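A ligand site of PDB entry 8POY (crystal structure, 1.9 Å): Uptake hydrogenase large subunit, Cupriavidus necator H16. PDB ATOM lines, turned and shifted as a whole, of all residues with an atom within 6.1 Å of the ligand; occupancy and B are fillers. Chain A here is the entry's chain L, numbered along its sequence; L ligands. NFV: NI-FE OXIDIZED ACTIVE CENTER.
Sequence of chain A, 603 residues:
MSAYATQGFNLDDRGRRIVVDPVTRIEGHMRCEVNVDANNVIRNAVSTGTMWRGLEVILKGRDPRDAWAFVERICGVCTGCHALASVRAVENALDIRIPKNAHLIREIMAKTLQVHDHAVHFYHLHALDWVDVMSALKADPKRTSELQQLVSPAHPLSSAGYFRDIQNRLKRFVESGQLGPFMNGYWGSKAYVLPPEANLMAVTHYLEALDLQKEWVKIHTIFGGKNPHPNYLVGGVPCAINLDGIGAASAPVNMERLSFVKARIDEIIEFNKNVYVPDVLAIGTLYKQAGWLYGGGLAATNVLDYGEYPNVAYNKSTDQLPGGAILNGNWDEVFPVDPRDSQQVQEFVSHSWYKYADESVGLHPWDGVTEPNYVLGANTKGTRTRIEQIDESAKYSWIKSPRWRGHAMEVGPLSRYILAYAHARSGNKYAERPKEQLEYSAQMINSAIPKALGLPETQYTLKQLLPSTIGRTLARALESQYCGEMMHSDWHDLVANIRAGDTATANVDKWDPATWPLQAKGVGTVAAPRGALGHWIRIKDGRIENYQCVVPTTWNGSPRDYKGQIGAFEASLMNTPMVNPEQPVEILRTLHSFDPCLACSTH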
ATOM      1  N   GLU A  27      19.557 -10.795  -6.726  1.00  0.00           N
ATOM      2  CA  GLU A  27      20.246 -11.881  -7.398  1.00  0.00           C
ATOM      3  C   GLU A  27      21.619 -11.369  -7.815  1.00  0.00           C
ATOM      4  O   GLU A  27      21.741 -10.259  -8.365  1.00  0.00           O
ATOM      5  CB  GLU A  27      19.471 -12.390  -8.608  1.00  0.00           C
ATOM      6  CG  GLU A  27      20.025 -13.676  -9.211  1.00  0.00           C
ATOM      7  CD  GLU A  27      21.333 -13.483  -9.965  1.00  0.00           C
ATOM      8  OE1 GLU A  27      21.552 -12.371 -10.513  1.00  0.00           O
ATOM      9  OE2 GLU A  27      22.159 -14.436 -10.022  1.00  0.00           O
ATOM     10  N   ILE A  74      21.613 -17.801 -17.929  1.00  0.00           N
ATOM     11  CA  ILE A  74      21.935 -16.448 -17.511  1.00  0.00           C
ATOM     12  C   ILE A  74      21.347 -16.227 -16.112  1.00  0.00           C
ATOM     13  O   ILE A  74      21.973 -15.577 -15.274  1.00  0.00           O
ATOM     14  CB  ILE A  74      21.425 -15.374 -18.502  1.00  0.00           C
ATOM     15  CG1 ILE A  74      22.288 -15.392 -19.767  1.00  0.00           C
ATOM     16  CG2 ILE A  74      21.452 -13.982 -17.882  1.00  0.00           C
ATOM     17  CD1 ILE A  74      21.706 -14.624 -20.940  1.00  0.00           C
ATOM     18  N   CYS A  75      20.167 -16.780 -15.848  1.00  0.00           N
ATOM     19  CA  CYS A  75      19.490 -16.531 -14.581  1.00  0.00           C
ATOM     20  C   CYS A  75      18.430 -17.576 -14.181  1.00  0.00           C
ATOM     21  O   CYS A  75      17.516 -17.887 -14.939  1.00  0.00           O
ATOM     22  CB  CYS A  75      18.837 -15.158 -14.603  1.00  0.00           C
ATOM     23  SG  CYS A  75      18.225 -14.668 -12.994  1.00  0.00           S
ATOM     24  N   GLY A  76      18.551 -18.071 -12.950  1.00  0.00           N
ATOM     25  CA  GLY A  76      17.604 -19.035 -12.414  1.00  0.00           C
ATOM     26  C   GLY A  76      16.465 -18.361 -11.666  1.00  0.00           C
ATOM     27  O   GLY A  76      15.535 -19.038 -11.227  1.00  0.00           O
ATOM     28  N   VAL A  77      16.536 -17.038 -11.511  1.00  0.00           N
ATOM     29  CA  VAL A  77      15.460 -16.276 -10.881  1.00  0.00           C
ATOM     30  C   VAL A  77      14.425 -15.888 -11.947  1.00  0.00           C
ATOM     31  O   VAL A  77      13.268 -16.250 -11.826  1.00  0.00           O
ATOM     32  CB  VAL A  77      15.985 -15.029 -10.139  1.00  0.00           C
ATOM     33  CG1 VAL A  77      14.823 -14.190  -9.639  1.00  0.00           C
ATOM     34  CG2 VAL A  77      16.898 -15.431  -8.964  1.00  0.00           C
ATOM     35  N   CYS A  78      14.840 -15.183 -13.002  1.00  0.00           N
ATOM     36  CA  CYS A  78      13.939 -14.907 -14.132  1.00  0.00           C
ATOM     37  C   CYS A  78      13.997 -16.068 -15.110  1.00  0.00           C
ATOM     38  O   CYS A  78      14.200 -15.916 -16.327  1.00  0.00           O
ATOM     39  CB  CYS A  78      14.287 -13.579 -14.786  1.00  0.00           C
ATOM     40  SG  CYS A  78      15.985 -13.453 -15.310  1.00  0.00           S
ATOM     41  N   THR A  79      13.763 -17.250 -14.547  1.00  0.00           N
ATOM     42  CA  THR A  79      14.016 -18.516 -15.234  1.00  0.00           C
ATOM     43  C   THR A  79      13.033 -18.766 -16.378  1.00  0.00           C
ATOM     44  O   THR A  79      11.820 -18.768 -16.190  1.00  0.00           O
ATOM     45  CB  THR A  79      14.049 -19.702 -14.241  1.00  0.00           C
ATOM     46  OG1 THR A  79      14.428 -20.892 -14.943  1.00  0.00           O
ATOM     47  CG2 THR A  79      12.673 -19.934 -13.532  1.00  0.00           C
ATOM     48  N   CYS A  81      12.720 -16.782 -19.144  1.00  0.00           N
ATOM     49  CA  CYS A  81      12.502 -15.595 -19.960  1.00  0.00           C
ATOM     50  C   CYS A  81      13.578 -15.442 -21.038  1.00  0.00           C
ATOM     51  O   CYS A  81      13.276 -15.037 -22.146  1.00  0.00           O
ATOM     52  CB  CYS A  81      12.361 -14.324 -19.095  1.00  0.00           C
ATOM     53  SG  CYS A  81      13.867 -13.656 -18.376  1.00  0.00           S
ATOM     54  N   HIS A  82      14.812 -15.799 -20.703  1.00  0.00           N
ATOM     55  CA  HIS A  82      15.893 -15.843 -21.689  1.00  0.00           C
ATOM     56  C   HIS A  82      15.683 -16.955 -22.709  1.00  0.00           C
ATOM     57  O   HIS A  82      16.013 -16.807 -23.892  1.00  0.00           O
ATOM     58  CB  HIS A  82      17.245 -16.017 -21.003  1.00  0.00           C
ATOM     59  CG  HIS A  82      17.672 -14.829 -20.198  1.00  0.00           C
ATOM     60  ND1 HIS A  82      18.121 -13.662 -20.788  1.00  0.00           N
ATOM     61  CD2 HIS A  82      17.702 -14.599 -18.863  1.00  0.00           C
ATOM     62  CE1 HIS A  82      18.426 -12.781 -19.847  1.00  0.00           C
ATOM     63  NE2 HIS A  82      18.160 -13.325 -18.671  1.00  0.00           N
ATOM     64  N   ASP A 117       8.058 -14.650  -9.671  1.00  0.00           N
ATOM     65  CA  ASP A 117       9.185 -13.747  -9.524  1.00  0.00           C
ATOM     66  C   ASP A 117       8.788 -12.519  -8.685  1.00  0.00           C
ATOM     67  O   ASP A 117       9.447 -12.209  -7.690  1.00  0.00           O
ATOM     68  CB  ASP A 117       9.723 -13.327 -10.905  1.00  0.00           C
ATOM     69  CG  ASP A 117      11.205 -13.019 -10.898  1.00  0.00           C
ATOM     70  OD1 ASP A 117      11.740 -12.608  -9.837  1.00  0.00           O
ATOM     71  OD2 ASP A 117      11.847 -13.170 -11.965  1.00  0.00           O
ATOM     72  N   ALA A 528      10.180  -9.224 -19.696  1.00  0.00           N
ATOM     73  CA  ALA A 528      10.656  -9.980 -18.550  1.00  0.00           C
ATOM     74  C   ALA A 528      10.215  -9.322 -17.222  1.00  0.00           C
ATOM     75  O   ALA A 528       9.849  -8.139 -17.216  1.00  0.00           O
ATOM     76  CB  ALA A 528      12.173 -10.092 -18.613  1.00  0.00           C
ATOM     77  N   PRO A 529      10.215 -10.079 -16.107  1.00  0.00           N
ATOM     78  CA  PRO A 529       9.772  -9.537 -14.820  1.00  0.00           C
ATOM     79  C   PRO A 529      10.349  -8.155 -14.467  1.00  0.00           C
ATOM     80  O   PRO A 529       9.654  -7.339 -13.873  1.00  0.00           O
ATOM     81  CB  PRO A 529      10.201 -10.603 -13.819  1.00  0.00           C
ATOM     82  CG  PRO A 529      10.099 -11.868 -14.593  1.00  0.00           C
ATOM     83  CD  PRO A 529      10.427 -11.544 -16.024  1.00  0.00           C
ATOM     84  N   ARG A 530      11.591  -7.906 -14.876  1.00  0.00           N
ATOM     85  CA  ARG A 530      12.303  -6.701 -14.491  1.00  0.00           C
ATOM     86  C   ARG A 530      12.325  -5.612 -15.560  1.00  0.00           C
ATOM     87  O   ARG A 530      12.832  -4.536 -15.306  1.00  0.00           O
ATOM     88  CB  ARG A 530      13.733  -7.061 -14.084  1.00  0.00           C
ATOM     89  CG  ARG A 530      13.773  -7.702 -12.713  1.00  0.00           C
ATOM     90  CD  ARG A 530      15.003  -8.560 -12.514  1.00  0.00           C
ATOM     91  NE  ARG A 530      14.862  -9.335 -11.274  1.00  0.00           N
ATOM     92  CZ  ARG A 530      14.157 -10.456 -11.155  1.00  0.00           C
ATOM     93  NH1 ARG A 530      13.540 -11.002 -12.202  1.00  0.00           N
ATOM     94  NH2 ARG A 530      14.086 -11.060  -9.976  1.00  0.00           N
ATOM     95  N   GLY A 531      11.769  -5.898 -16.735  1.00  0.00           N
ATOM     96  CA  GLY A 531      11.658  -4.892 -17.790  1.00  0.00           C
ATOM     97  C   GLY A 531      11.883  -5.440 -19.193  1.00  0.00           C
ATOM     98  O   GLY A 531      11.575  -6.595 -19.480  1.00  0.00           O
ATOM     99  N   LEU A 533      13.567  -7.001 -22.196  1.00  0.00           N
ATOM    100  CA  LEU A 533      14.610  -7.965 -22.531  1.00  0.00           C
ATOM    101  C   LEU A 533      14.657  -8.195 -24.028  1.00  0.00           C
ATOM    102  O   LEU A 533      13.612  -8.361 -24.668  1.00  0.00           O
ATOM    103  CB  LEU A 533      14.357  -9.312 -21.838  1.00  0.00           C
ATOM    104  CG  LEU A 533      15.237 -10.485 -22.315  1.00  0.00           C
ATOM    105  CD1 LEU A 533      16.700 -10.280 -21.938  1.00  0.00           C
ATOM    106  CD2 LEU A 533      14.713 -11.801 -21.770  1.00  0.00           C
ATOM    107  N   HIS A 535      17.126 -10.428 -27.106  1.00  0.00           N
ATOM    108  CA  HIS A 535      18.252 -11.223 -27.617  1.00  0.00           C
ATOM    109  C   HIS A 535      18.362 -10.974 -29.107  1.00  0.00           C
ATOM    110  O   HIS A 535      17.375 -11.094 -29.838  1.00  0.00           O
ATOM    111  CB  HIS A 535      18.014 -12.707 -27.392  1.00  0.00           C
ATOM    112  CG  HIS A 535      18.108 -13.133 -25.967  1.00  0.00           C
ATOM    113  ND1 HIS A 535      18.368 -14.431 -25.602  1.00  0.00           N
ATOM    114  CD2 HIS A 535      17.953 -12.437 -24.819  1.00  0.00           C
ATOM    115  CE1 HIS A 535      18.380 -14.519 -24.283  1.00  0.00           C
ATOM    116  NE2 HIS A 535      18.123 -13.314 -23.785  1.00  0.00           N
ATOM    117  N   VAL A 551      19.509  -6.765 -21.340  1.00  0.00           N
ATOM    118  CA  VAL A 551      18.683  -7.380 -20.313  1.00  0.00           C
ATOM    119  C   VAL A 551      18.151  -6.261 -19.403  1.00  0.00           C
ATOM    120  O   VAL A 551      18.755  -5.194 -19.334  1.00  0.00           O
ATOM    121  CB  VAL A 551      19.541  -8.428 -19.579  1.00  0.00           C
ATOM    122  CG1 VAL A 551      18.752  -9.213 -18.554  1.00  0.00           C
ATOM    123  CG2 VAL A 551      20.147  -9.394 -20.587  1.00  0.00           C
ATOM    124  N   PRO A 552      16.976  -6.460 -18.761  1.00  0.00           N
ATOM    125  CA  PRO A 552      16.366  -5.344 -18.040  1.00  0.00           C
ATOM    126  C   PRO A 552      17.262  -4.657 -17.015  1.00  0.00           C
ATOM    127  O   PRO A 552      17.296  -3.409 -16.949  1.00  0.00           O
ATOM    128  CB  PRO A 552      15.175  -5.995 -17.358  1.00  0.00           C
ATOM    129  CG  PRO A 552      14.788  -7.072 -18.295  1.00  0.00           C
ATOM    130  CD  PRO A 552      16.037  -7.587 -18.898  1.00  0.00           C
ATOM    131  N   THR A 553      17.996  -5.443 -16.232  1.00  0.00           N
ATOM    132  CA  THR A 553      18.840  -4.888 -15.191  1.00  0.00           C
ATOM    133  C   THR A 553      20.100  -4.264 -15.829  1.00  0.00           C
ATOM    134  O   THR A 553      20.733  -3.427 -15.214  1.00  0.00           O
ATOM    135  CB  THR A 553      19.159  -5.937 -14.092  1.00  0.00           C
ATOM    136  OG1 THR A 553      17.946  -6.469 -13.540  1.00  0.00           O
ATOM    137  CG2 THR A 553      19.962  -5.303 -12.943  1.00  0.00           C
ATOM    138  N   THR A 554      20.433  -4.659 -17.065  1.00  0.00           N
ATOM    139  CA  THR A 554      21.459  -3.945 -17.844  1.00  0.00           C
ATOM    140  C   THR A 554      21.019  -2.489 -18.054  1.00  0.00           C
ATOM    141  O   THR A 554      21.802  -1.569 -17.856  1.00  0.00           O
ATOM    142  CB  THR A 554      21.744  -4.588 -19.215  1.00  0.00           C
ATOM    143  OG1 THR A 554      21.872  -6.002 -19.084  1.00  0.00           O
ATOM    144  CG2 THR A 554      23.013  -4.015 -19.836  1.00  0.00           C
ATOM    145  N   ASP A 595      14.159  -4.570  -8.277  1.00  0.00           N
ATOM    146  CA  ASP A 595      14.368  -6.019  -8.292  1.00  0.00           C
ATOM    147  C   ASP A 595      15.646  -6.363  -9.074  1.00  0.00           C
ATOM    148  O   ASP A 595      15.584  -7.027 -10.113  1.00  0.00           O
ATOM    149  CB  ASP A 595      13.134  -6.696  -8.899  1.00  0.00           C
ATOM    150  CG  ASP A 595      13.129  -8.191  -8.717  1.00  0.00           C
ATOM    151  OD1 ASP A 595      14.140  -8.790  -8.292  1.00  0.00           O
ATOM    152  OD2 ASP A 595      12.077  -8.793  -8.986  1.00  0.00           O
ATOM    153  N   PRO A 596      16.811  -5.897  -8.585  1.00  0.00           N
ATOM    154  CA  PRO A 596      18.017  -6.048  -9.399  1.00  0.00           C
ATOM    155  C   PRO A 596      18.428  -7.516  -9.571  1.00  0.00           C
ATOM    156  O   PRO A 596      18.488  -8.252  -8.599  1.00  0.00           O
ATOM    157  CB  PRO A 596      19.079  -5.268  -8.600  1.00  0.00           C
ATOM    158  CG  PRO A 596      18.313  -4.347  -7.728  1.00  0.00           C
ATOM    159  CD  PRO A 596      17.095  -5.149  -7.350  1.00  0.00           C
ATOM    160  N   CYS A 597      18.677  -7.909 -10.812  1.00  0.00           N
ATOM    161  CA  CYS A 597      19.232  -9.232 -11.111  1.00  0.00           C
ATOM    162  C   CYS A 597      20.569  -9.059 -11.827  1.00  0.00           C
ATOM    163  O   CYS A 597      20.619  -8.767 -13.030  1.00  0.00           O
ATOM    164  CB  CYS A 597      18.274 -10.052 -11.960  1.00  0.00           C
ATOM    165  SG  CYS A 597      18.814 -11.780 -12.157  1.00  0.00           S
ATOM    166  N   LEU A 598      21.644  -9.232 -11.076  1.00  0.00           N
ATOM    167  CA  LEU A 598      22.966  -8.857 -11.552  1.00  0.00           C
ATOM    168  C   LEU A 598      23.558  -9.866 -12.506  1.00  0.00           C
ATOM    169  O   LEU A 598      24.285  -9.493 -13.417  1.00  0.00           O
ATOM    170  CB  LEU A 598      23.918  -8.561 -10.394  1.00  0.00           C
ATOM    171  CG  LEU A 598      23.780  -7.162  -9.807  1.00  0.00           C
ATOM    172  CD1 LEU A 598      24.469  -6.113 -10.671  1.00  0.00           C
ATOM    173  CD2 LEU A 598      22.327  -6.764  -9.558  1.00  0.00           C
ATOM    174  N   ALA A 599      23.228 -11.150 -12.328  1.00  0.00           N
ATOM    175  CA  ALA A 599      23.630 -12.164 -13.300  1.00  0.00           C
ATOM    176  C   ALA A 599      22.994 -11.858 -14.655  1.00  0.00           C
ATOM    177  O   ALA A 599      23.636 -11.936 -15.704  1.00  0.00           O
ATOM    178  CB  ALA A 599      23.234 -13.545 -12.827  1.00  0.00           C
ATOM    179  N   CYS A 600      21.719 -11.497 -14.624  1.00  0.00           N
ATOM    180  CA  CYS A 600      21.019 -11.025 -15.801  1.00  0.00           C
ATOM    181  C   CYS A 600      21.690  -9.823 -16.428  1.00  0.00           C
ATOM    182  O   CYS A 600      21.867  -9.780 -17.649  1.00  0.00           O
ATOM    183  CB  CYS A 600      19.572 -10.649 -15.446  1.00  0.00           C
ATOM    184  SG  CYS A 600      18.393 -11.924 -15.868  1.00  0.00           S
ATOM    185  N   SER A 601      22.040  -8.841 -15.603  1.00  0.00           N
ATOM    186  CA  SER A 601      22.541  -7.571 -16.105  1.00  0.00           C
ATOM    187  C   SER A 601      23.851  -7.738 -16.870  1.00  0.00           C
ATOM    188  O   SER A 601      24.109  -7.004 -17.827  1.00  0.00           O
ATOM    189  CB  SER A 601      22.720  -6.557 -14.971  1.00  0.00           C
ATOM    190  OG  SER A 601      23.834  -6.883 -14.152  1.00  0.00           O
HETATM  191 FE   NFV L   1      16.194 -11.094 -15.718  1.00  0.00          FE
HETATM  192 NI   NFV L   1      17.349 -12.644 -13.568  1.00  0.00          NI
HETATM  193  C1  NFV L   1      16.019 -11.098 -17.548  1.00  0.00           C
HETATM  194  O1  NFV L   1      15.902 -11.077 -18.711  1.00  0.00           O
HETATM  195  C2  NFV L   1      16.782  -9.217 -15.680  1.00  0.00           C
HETATM  196  N2  NFV L   1      17.112  -8.161 -15.649  1.00  0.00           N
HETATM  197  C3  NFV L   1      14.342 -10.520 -15.513  1.00  0.00           C
HETATM  198  N3  NFV L   1      13.314 -10.230 -15.395  1.00  0.00           N
HETATM  199  O4  NFV L   1      16.342 -11.071 -13.746  1.00  0.00           O
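NI of the ligand is bound by SG of Cys 597, at 2.2 Å.
The side-chain sulfur (SG) of Cys 75 is bound to a nickel atom (NI) of the ligand.
The side-chain sulfur of Cys 600 is bound to an iron atom (FE) of the ligand, 2.4 Å away.
SG of Cys 78 binds NI of the ligand, at 2.4 Å.
N of Thr 553 lies within hydrogen-bond range of N2 of the ligand, 2.9 Å away.
The side-chain hydroxyl (OG1) of Thr 553 sits at hydrogen-bond distance from a nitrogen (N2) of the ligand (2.8 Å).
N of Arg 530 lies within hydrogen-bond range of N3 of the ligand (2.9 Å).
The guanidinium group of Arg 530 is in hydrogen-bond range of a nitrogen (N3) of the ligand, 3.3 Å away.
An oxygen (O1) of the ligand sits at hydrogen-bond distance from a ring nitrogen (NE2) of His 82 (3.2 Å).
An oxygen (O1) of the ligand lies within hydrogen-bond range of the side-chain sulfur (SG) of Cys 81 (3.3 Å).
SG of Cys 597 lies close to OE1 of Glu 27 (3.2 Å).
The side-chain sulfur (SG) of Cys 75 sits close to the backbone NH (N) of Val 77 (3.3 Å).
A ring nitrogen (NE2) of His 82 sits close to the side-chain sulfur (SG) of Cys 600 (3.1 Å).
The backbone carbonyl oxygen (O) of Cys 78 is in hydrogen-bond range of the side-chain sulfur (SG) of Cys 81, at 3.1 Å.
The side-chain carboxylate of Asp 117 lies within salt-bridge range of the guanidinium group of Arg 530.
The guanidinium group of Arg 530 is in salt-bridge range of the side-chain carboxylate of Asp 595, 2.8 Å away.
ND1 of His 82 sits at hydrogen-bond distance from NE2 of His 535, 3.0 Å away.
The backbone carbonyl oxygen of Val 551 lies close to the side-chain hydroxyl of Thr 554, 3.2 Å away.
N of Pro 529 lies close to N3 of the ligand (3.2 Å).
Ala 528 touches the ligand.
Leu 533 touches the ligand (CD2 to O1, 3.4 Å).
Val 551 touches the ligand.
Pro 552 touches the ligand (CB to N2, 3.4 Å).
Of the 27 residues printed, 13 come within 4 Å of the ligand.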
